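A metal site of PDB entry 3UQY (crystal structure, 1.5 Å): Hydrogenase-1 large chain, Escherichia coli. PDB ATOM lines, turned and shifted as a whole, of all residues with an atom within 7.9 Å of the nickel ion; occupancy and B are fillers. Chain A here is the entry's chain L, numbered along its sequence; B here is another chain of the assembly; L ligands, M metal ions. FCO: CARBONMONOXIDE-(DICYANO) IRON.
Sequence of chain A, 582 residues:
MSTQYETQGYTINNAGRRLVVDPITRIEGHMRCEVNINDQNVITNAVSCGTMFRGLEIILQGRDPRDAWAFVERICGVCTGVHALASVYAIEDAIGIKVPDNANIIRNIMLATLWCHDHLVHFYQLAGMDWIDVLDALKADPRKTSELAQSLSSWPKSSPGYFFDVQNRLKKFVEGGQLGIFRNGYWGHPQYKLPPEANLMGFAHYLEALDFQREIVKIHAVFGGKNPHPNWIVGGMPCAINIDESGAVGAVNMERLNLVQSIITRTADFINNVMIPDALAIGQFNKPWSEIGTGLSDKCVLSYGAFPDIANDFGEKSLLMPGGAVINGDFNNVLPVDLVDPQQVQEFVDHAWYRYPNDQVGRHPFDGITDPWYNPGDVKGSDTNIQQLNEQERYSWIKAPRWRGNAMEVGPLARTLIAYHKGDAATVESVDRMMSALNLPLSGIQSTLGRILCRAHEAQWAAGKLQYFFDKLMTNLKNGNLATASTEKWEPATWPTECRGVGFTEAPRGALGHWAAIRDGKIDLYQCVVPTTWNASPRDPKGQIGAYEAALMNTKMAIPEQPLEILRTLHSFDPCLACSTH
Within 4 Å of the nickel ion: Cys 76, Cys 79, Cys 576 and Cys 579. Along chain A the residues within 4 Å of the nickel ion span positions 76 to 579.
The nickel ion is bound by the side-chain sulfur (SG) of Cys 576, the side-chain sulfur (SG) of Cys 76, the side-chain sulfur (SG) of Cys 79 and the side-chain sulfur (SG) of Cys 579. The nickel ion has four donor atoms within binding distance.
The backbone NH of Val 78 lies close to the side-chain sulfur of Cys 76, at 3.4 Å. A ring nitrogen (NE2) of His 83 sits close to the side-chain sulfur of Cys 579, 3.2 Å away. OG1 of Thr 532 sits at hydrogen-bond distance from N of Cys 576, 3.1 Å away. The side-chain carboxylate (OE1) of Glu 28 sits close to the side-chain sulfur (SG) of Cys 576.
The side-chain sulfur (SG) of Cys 579 is bound to an iron atom (FE) of the ligand, at 2.3 Å. A nitrogen (N2) of the ligand is in hydrogen-bond range of the backbone NH (N) of Arg 509, 2.9 Å away. N of Thr 532 sits at hydrogen-bond distance from N1 of the ligand, 3.0 Å away. The side-chain hydroxyl (OG1) of Thr 532 is in hydrogen-bond range of a nitrogen (N1) of the ligand (2.8 Å). NE2 of His 83 sits at hydrogen-bond distance from O3 of the ligand. SG of Cys 79 binds FE of the ligand (2.3 Å). The guanidinium group (NH1) of Arg 509 sits at hydrogen-bond distance from a nitrogen (N2) of the ligand (3.2 Å).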
ATOM      1  N   GLU A  28     -25.881 -10.905 -12.219  1.00  0.00           N
ATOM      2  CA  GLU A  28     -24.515 -11.165 -11.761  1.00  0.00           C
ATOM      3  C   GLU A  28     -23.558 -10.675 -12.854  1.00  0.00           C
ATOM      4  O   GLU A  28     -23.757 -10.985 -14.048  1.00  0.00           O
ATOM      5  CB  GLU A  28     -24.309 -12.659 -11.503  1.00  0.00           C
ATOM      6  CG  GLU A  28     -22.994 -13.002 -10.810  1.00  0.00           C
ATOM      7  CD  GLU A  28     -21.785 -12.777 -11.694  1.00  0.00           C
ATOM      8  OE1 GLU A  28     -21.883 -13.070 -12.895  1.00  0.00           O
ATOM      9  OE2 GLU A  28     -20.750 -12.289 -11.192  1.00  0.00           O
ATOM     10  N   GLU A  73     -15.266 -23.488  -9.067  1.00  0.00           N
ATOM     11  CA  GLU A  73     -16.365 -23.008  -8.231  1.00  0.00           C
ATOM     12  C   GLU A  73     -16.423 -21.492  -8.267  1.00  0.00           C
ATOM     13  O   GLU A  73     -17.522 -20.909  -8.244  1.00  0.00           O
ATOM     14  CB  GLU A  73     -16.285 -23.536  -6.794  1.00  0.00           C
ATOM     15  CG  GLU A  73     -17.554 -23.227  -5.994  1.00  0.00           C
ATOM     16  CD  GLU A  73     -17.637 -24.031  -4.717  1.00  0.00           C
ATOM     17  OE1 GLU A  73     -16.685 -23.993  -3.914  1.00  0.00           O
ATOM     18  OE2 GLU A  73     -18.670 -24.695  -4.485  1.00  0.00           O
ATOM     19  N   ILE A  75     -15.948 -19.597 -10.642  1.00  0.00           N
ATOM     20  CA  ILE A  75     -16.559 -19.009 -11.831  1.00  0.00           C
ATOM     21  C   ILE A  75     -17.726 -18.112 -11.393  1.00  0.00           C
ATOM     22  O   ILE A  75     -17.992 -17.092 -12.011  1.00  0.00           O
ATOM     23  CB  ILE A  75     -17.023 -20.089 -12.857  1.00  0.00           C
ATOM     24  CG1 ILE A  75     -15.795 -20.636 -13.601  1.00  0.00           C
ATOM     25  CG2 ILE A  75     -17.987 -19.486 -13.867  1.00  0.00           C
ATOM     26  CD1 ILE A  75     -16.065 -21.926 -14.351  1.00  0.00           C
ATOM     27  N   CYS A  76     -18.418 -18.505 -10.325  1.00  0.00           N
ATOM     28  CA  CYS A  76     -19.604 -17.773  -9.926  1.00  0.00           C
ATOM     29  C   CYS A  76     -20.015 -17.996  -8.488  1.00  0.00           C
ATOM     30  O   CYS A  76     -20.146 -19.134  -8.041  1.00  0.00           O
ATOM     31  CB  CYS A  76     -20.772 -18.139 -10.852  1.00  0.00           C
ATOM     32  SG  CYS A  76     -22.234 -17.133 -10.561  1.00  0.00           S
ATOM     33  N   GLY A  77     -20.259 -16.899  -7.780  1.00  0.00           N
ATOM     34  CA  GLY A  77     -20.669 -16.945  -6.381  1.00  0.00           C
ATOM     35  C   GLY A  77     -22.176 -16.889  -6.188  1.00  0.00           C
ATOM     36  O   GLY A  77     -22.663 -17.038  -5.070  1.00  0.00           O
ATOM     37  N   VAL A  78     -22.903 -16.664  -7.272  1.00  0.00           N
ATOM     38  CA  VAL A  78     -24.367 -16.691  -7.274  1.00  0.00           C
ATOM     39  C   VAL A  78     -24.818 -18.145  -7.463  1.00  0.00           C
ATOM     40  O   VAL A  78     -25.469 -18.716  -6.589  1.00  0.00           O
ATOM     41  CB  VAL A  78     -24.956 -15.708  -8.345  1.00  0.00           C
ATOM     42  CG1 VAL A  78     -26.481 -15.801  -8.337  1.00  0.00           C
ATOM     43  CG2 VAL A  78     -24.506 -14.263  -8.040  1.00  0.00           C
ATOM     44  N   CYS A  79     -24.440 -18.761  -8.588  1.00  0.00           N
ATOM     45  CA  CYS A  79     -24.669 -20.196  -8.756  1.00  0.00           C
ATOM     46  C   CYS A  79     -23.535 -20.987  -8.072  1.00  0.00           C
ATOM     47  O   CYS A  79     -22.918 -21.889  -8.644  1.00  0.00           O
ATOM     48  CB  CYS A  79     -24.899 -20.587 -10.222  1.00  0.00           C
ATOM     49  SG  CYS A  79     -23.555 -20.157 -11.385  1.00  0.00           S
ATOM     50  N   THR A  80     -23.287 -20.637  -6.822  1.00  0.00           N
ATOM     51  CA  THR A  80     -22.178 -21.215  -6.093  1.00  0.00           C
ATOM     52  C   THR A  80     -22.361 -22.718  -5.821  1.00  0.00           C
ATOM     53  O   THR A  80     -23.357 -23.153  -5.243  1.00  0.00           O
ATOM     54  CB  THR A  80     -21.863 -20.441  -4.790  1.00  0.00           C
ATOM     55  OG1 THR A  80     -20.740 -21.061  -4.150  1.00  0.00           O
ATOM     56  CG2 THR A  80     -23.062 -20.440  -3.815  1.00  0.00           C
ATOM     57  N   VAL A  82     -22.393 -25.100  -8.274  1.00  0.00           N
ATOM     58  CA  VAL A  82     -22.750 -25.850  -9.479  1.00  0.00           C
ATOM     59  C   VAL A  82     -21.523 -26.221 -10.337  1.00  0.00           C
ATOM     60  O   VAL A  82     -21.464 -27.319 -10.912  1.00  0.00           O
ATOM     61  CB  VAL A  82     -23.867 -25.202 -10.314  1.00  0.00           C
ATOM     62  CG1 VAL A  82     -23.375 -23.982 -11.120  1.00  0.00           C
ATOM     63  CG2 VAL A  82     -24.539 -26.274 -11.192  1.00  0.00           C
ATOM     64  N   HIS A  83     -20.542 -25.318 -10.399  1.00  0.00           N
ATOM     65  CA  HIS A  83     -19.321 -25.599 -11.156  1.00  0.00           C
ATOM     66  C   HIS A  83     -18.441 -26.623 -10.450  1.00  0.00           C
ATOM     67  O   HIS A  83     -17.721 -27.408 -11.104  1.00  0.00           O
ATOM     68  CB  HIS A  83     -18.555 -24.298 -11.442  1.00  0.00           C
ATOM     69  CG  HIS A  83     -19.260 -23.416 -12.409  1.00  0.00           C
ATOM     70  ND1 HIS A  83     -19.298 -23.680 -13.767  1.00  0.00           N
ATOM     71  CD2 HIS A  83     -19.955 -22.263 -12.229  1.00  0.00           C
ATOM     72  CE1 HIS A  83     -19.985 -22.723 -14.382  1.00  0.00           C
ATOM     73  NE2 HIS A  83     -20.407 -21.867 -13.469  1.00  0.00           N
ATOM     74  N   LEU A 114     -29.122 -25.111  -3.819  1.00  0.00           N
ATOM     75  CA  LEU A 114     -28.772 -23.994  -4.701  1.00  0.00           C
ATOM     76  C   LEU A 114     -29.953 -23.539  -5.553  1.00  0.00           C
ATOM     77  O   LEU A 114     -30.225 -22.358  -5.649  1.00  0.00           O
ATOM     78  CB  LEU A 114     -27.564 -24.335  -5.581  1.00  0.00           C
ATOM     79  CG  LEU A 114     -27.127 -23.230  -6.557  1.00  0.00           C
ATOM     80  CD1 LEU A 114     -26.663 -21.965  -5.760  1.00  0.00           C
ATOM     81  CD2 LEU A 114     -26.029 -23.719  -7.480  1.00  0.00           C
ATOM     82  N   ASP A 118     -31.046 -19.764  -5.125  1.00  0.00           N
ATOM     83  CA  ASP A 118     -30.756 -18.917  -6.263  1.00  0.00           C
ATOM     84  C   ASP A 118     -32.075 -18.424  -6.884  1.00  0.00           C
ATOM     85  O   ASP A 118     -32.252 -17.241  -7.174  1.00  0.00           O
ATOM     86  CB  ASP A 118     -29.942 -19.753  -7.271  1.00  0.00           C
ATOM     87  CG  ASP A 118     -29.198 -18.904  -8.274  1.00  0.00           C
ATOM     88  OD1 ASP A 118     -29.715 -17.825  -8.661  1.00  0.00           O
ATOM     89  OD2 ASP A 118     -28.094 -19.351  -8.707  1.00  0.00           O
ATOM     90  N   ALA A 507     -27.695 -26.198 -14.053  1.00  0.00           N
ATOM     91  CA  ALA A 507     -27.562 -25.114 -13.099  1.00  0.00           C
ATOM     92  C   ALA A 507     -28.879 -24.353 -13.014  1.00  0.00           C
ATOM     93  O   ALA A 507     -29.739 -24.516 -13.876  1.00  0.00           O
ATOM     94  CB  ALA A 507     -26.434 -24.203 -13.540  1.00  0.00           C
ATOM     95  N   PRO A 508     -29.046 -23.482 -12.006  1.00  0.00           N
ATOM     96  CA  PRO A 508     -30.275 -22.671 -11.968  1.00  0.00           C
ATOM     97  C   PRO A 508     -30.631 -22.003 -13.316  1.00  0.00           C
ATOM     98  O   PRO A 508     -31.814 -21.900 -13.651  1.00  0.00           O
ATOM     99  CB  PRO A 508     -29.965 -21.631 -10.881  1.00  0.00           C
ATOM    100  CG  PRO A 508     -29.094 -22.414  -9.927  1.00  0.00           C
ATOM    101  CD  PRO A 508     -28.206 -23.252 -10.816  1.00  0.00           C
ATOM    102  N   ARG A 509     -29.623 -21.586 -14.075  1.00  0.00           N
ATOM    103  CA  ARG A 509     -29.841 -20.853 -15.323  1.00  0.00           C
ATOM    104  C   ARG A 509     -29.844 -21.710 -16.596  1.00  0.00           C
ATOM    105  O   ARG A 509     -30.125 -21.185 -17.681  1.00  0.00           O
ATOM    106  CB  ARG A 509     -28.816 -19.711 -15.452  1.00  0.00           C
ATOM    107  CG  ARG A 509     -29.065 -18.639 -14.398  1.00  0.00           C
ATOM    108  CD  ARG A 509     -27.825 -17.792 -14.089  1.00  0.00           C
ATOM    109  NE  ARG A 509     -28.188 -16.888 -12.998  1.00  0.00           N
ATOM    110  CZ  ARG A 509     -28.143 -17.186 -11.697  1.00  0.00           C
ATOM    111  NH1 ARG A 509     -27.669 -18.360 -11.279  1.00  0.00           N
ATOM    112  NH2 ARG A 509     -28.576 -16.296 -10.792  1.00  0.00           N
ATOM    113  N   VAL A 530     -21.343 -22.689 -20.429  1.00  0.00           N
ATOM    114  CA  VAL A 530     -22.153 -22.390 -19.249  1.00  0.00           C
ATOM    115  C   VAL A 530     -23.526 -21.863 -19.720  1.00  0.00           C
ATOM    116  O   VAL A 530     -23.647 -21.386 -20.849  1.00  0.00           O
ATOM    117  CB  VAL A 530     -21.356 -21.405 -18.360  1.00  0.00           C
ATOM    118  CG1 VAL A 530     -21.994 -21.186 -17.023  1.00  0.00           C
ATOM    119  CG2 VAL A 530     -19.935 -21.961 -18.135  1.00  0.00           C
ATOM    120  N   PRO A 531     -24.594 -21.997 -18.880  1.00  0.00           N
ATOM    121  CA  PRO A 531     -25.922 -21.653 -19.405  1.00  0.00           C
ATOM    122  C   PRO A 531     -26.019 -20.251 -19.989  1.00  0.00           C
ATOM    123  O   PRO A 531     -26.555 -20.087 -21.089  1.00  0.00           O
ATOM    124  CB  PRO A 531     -26.854 -21.813 -18.185  1.00  0.00           C
ATOM    125  CG  PRO A 531     -26.043 -22.380 -17.089  1.00  0.00           C
ATOM    126  CD  PRO A 531     -24.692 -22.769 -17.634  1.00  0.00           C
ATOM    127  N   THR A 532     -25.468 -19.243 -19.313  1.00  0.00           N
ATOM    128  CA  THR A 532     -25.579 -17.884 -19.845  1.00  0.00           C
ATOM    129  C   THR A 532     -24.692 -17.720 -21.090  1.00  0.00           C
ATOM    130  O   THR A 532     -24.950 -16.839 -21.904  1.00  0.00           O
ATOM    131  CB  THR A 532     -25.322 -16.820 -18.738  1.00  0.00           C
ATOM    132  OG1 THR A 532     -26.285 -16.993 -17.691  1.00  0.00           O
ATOM    133  CG2 THR A 532     -25.475 -15.395 -19.293  1.00  0.00           C
ATOM    134  N   ASP A 574     -32.409 -14.469 -16.072  1.00  0.00           N
ATOM    135  CA  ASP A 574     -31.530 -14.552 -14.911  1.00  0.00           C
ATOM    136  C   ASP A 574     -30.047 -14.567 -15.370  1.00  0.00           C
ATOM    137  O   ASP A 574     -29.323 -15.536 -15.141  1.00  0.00           O
ATOM    138  CB  ASP A 574     -31.921 -15.816 -14.124  1.00  0.00           C
ATOM    139  CG  ASP A 574     -31.197 -15.973 -12.813  1.00  0.00           C
ATOM    140  OD1 ASP A 574     -30.488 -15.033 -12.345  1.00  0.00           O
ATOM    141  OD2 ASP A 574     -31.366 -17.076 -12.233  1.00  0.00           O
ATOM    142  N   PRO A 575     -29.596 -13.484 -16.025  1.00  0.00           N
ATOM    143  CA  PRO A 575     -28.238 -13.487 -16.608  1.00  0.00           C
ATOM    144  C   PRO A 575     -27.129 -13.607 -15.541  1.00  0.00           C
ATOM    145  O   PRO A 575     -27.173 -12.926 -14.532  1.00  0.00           O
ATOM    146  CB  PRO A 575     -28.134 -12.116 -17.294  1.00  0.00           C
ATOM    147  CG  PRO A 575     -29.565 -11.727 -17.555  1.00  0.00           C
ATOM    148  CD  PRO A 575     -30.333 -12.253 -16.366  1.00  0.00           C
ATOM    149  N   CYS A 576     -26.147 -14.471 -15.817  1.00  0.00           N
ATOM    150  CA  CYS A 576     -24.997 -14.599 -14.953  1.00  0.00           C
ATOM    151  C   CYS A 576     -23.774 -14.432 -15.822  1.00  0.00           C
ATOM    152  O   CYS A 576     -23.373 -15.367 -16.533  1.00  0.00           O
ATOM    153  CB  CYS A 576     -24.988 -15.965 -14.283  1.00  0.00           C
ATOM    154  SG  CYS A 576     -23.749 -16.056 -12.966  1.00  0.00           S
ATOM    155  N   LEU A 577     -23.185 -13.244 -15.792  1.00  0.00           N
ATOM    156  CA  LEU A 577     -22.184 -12.894 -16.781  1.00  0.00           C
ATOM    157  C   LEU A 577     -20.808 -13.444 -16.463  1.00  0.00           C
ATOM    158  O   LEU A 577     -20.053 -13.761 -17.376  1.00  0.00           O
ATOM    159  CB  LEU A 577     -22.182 -11.382 -17.044  1.00  0.00           C
ATOM    160  CG  LEU A 577     -23.234 -10.887 -18.061  1.00  0.00           C
ATOM    161  CD1 LEU A 577     -22.857 -11.253 -19.510  1.00  0.00           C
ATOM    162  CD2 LEU A 577     -24.651 -11.346 -17.718  1.00  0.00           C
ATOM    163  N   ALA A 578     -20.503 -13.598 -15.168  1.00  0.00           N
ATOM    164  CA  ALA A 578     -19.245 -14.233 -14.766  1.00  0.00           C
ATOM    165  C   ALA A 578     -19.278 -15.695 -15.208  1.00  0.00           C
ATOM    166  O   ALA A 578     -18.270 -16.214 -15.706  1.00  0.00           O
ATOM    167  CB  ALA A 578     -19.026 -14.112 -13.261  1.00  0.00           C
ATOM    168  N   CYS A 579     -20.433 -16.330 -15.051  1.00  0.00           N
ATOM    169  CA  CYS A 579     -20.647 -17.657 -15.610  1.00  0.00           C
ATOM    170  C   CYS A 579     -20.434 -17.708 -17.112  1.00  0.00           C
ATOM    171  O   CYS A 579     -19.738 -18.601 -17.614  1.00  0.00           O
ATOM    172  CB  CYS A 579     -22.055 -18.170 -15.307  1.00  0.00           C
ATOM    173  SG  CYS A 579     -22.144 -19.162 -13.824  1.00  0.00           S
ATOM    174  N   SER A 580     -21.019 -16.745 -17.822  1.00  0.00           N
ATOM    175  CA  SER A 580     -21.046 -16.826 -19.289  1.00  0.00           C
ATOM    176  C   SER A 580     -19.655 -16.732 -19.906  1.00  0.00           C
ATOM    177  O   SER A 580     -19.402 -17.311 -20.967  1.00  0.00           O
ATOM    178  CB  SER A 580     -21.927 -15.708 -19.869  1.00  0.00           C
ATOM    179  OG  SER A 580     -21.279 -14.447 -19.795  1.00  0.00           O
ATOM    180  N   CYS B  17     -16.659 -12.858  -8.965  1.00  0.00           N
ATOM    181  CA  CYS B  17     -17.697 -13.884  -9.117  1.00  0.00           C
ATOM    182  C   CYS B  17     -18.976 -13.523  -8.351  1.00  0.00           C
ATOM    183  O   CYS B  17     -19.986 -14.226  -8.472  1.00  0.00           O
ATOM    184  CB  CYS B  17     -17.189 -15.255  -8.684  1.00  0.00           C
ATOM    185  SG  CYS B  17     -17.346 -15.537  -6.899  1.00  0.00           S
HETATM  186 FE   FCO L   1     -24.211 -20.055 -13.550  1.00  0.00          FE
HETATM  187  C1  FCO L   1     -24.790 -19.502 -15.280  1.00  0.00           C
HETATM  188  N1  FCO L   1     -25.147 -19.161 -16.330  1.00  0.00           N
HETATM  189  C2  FCO L   1     -25.983 -20.644 -13.154  1.00  0.00           C
HETATM  190  N2  FCO L   1     -27.062 -21.001 -12.907  1.00  0.00           N
HETATM  191  C3  FCO L   1     -23.816 -21.668 -14.100  1.00  0.00           C
HETATM  192  O3  FCO L   1     -23.546 -22.720 -14.470  1.00  0.00           O
HETATM  193 NI    NI M   1     -23.584 -18.028 -12.122  1.00  0.00          NI
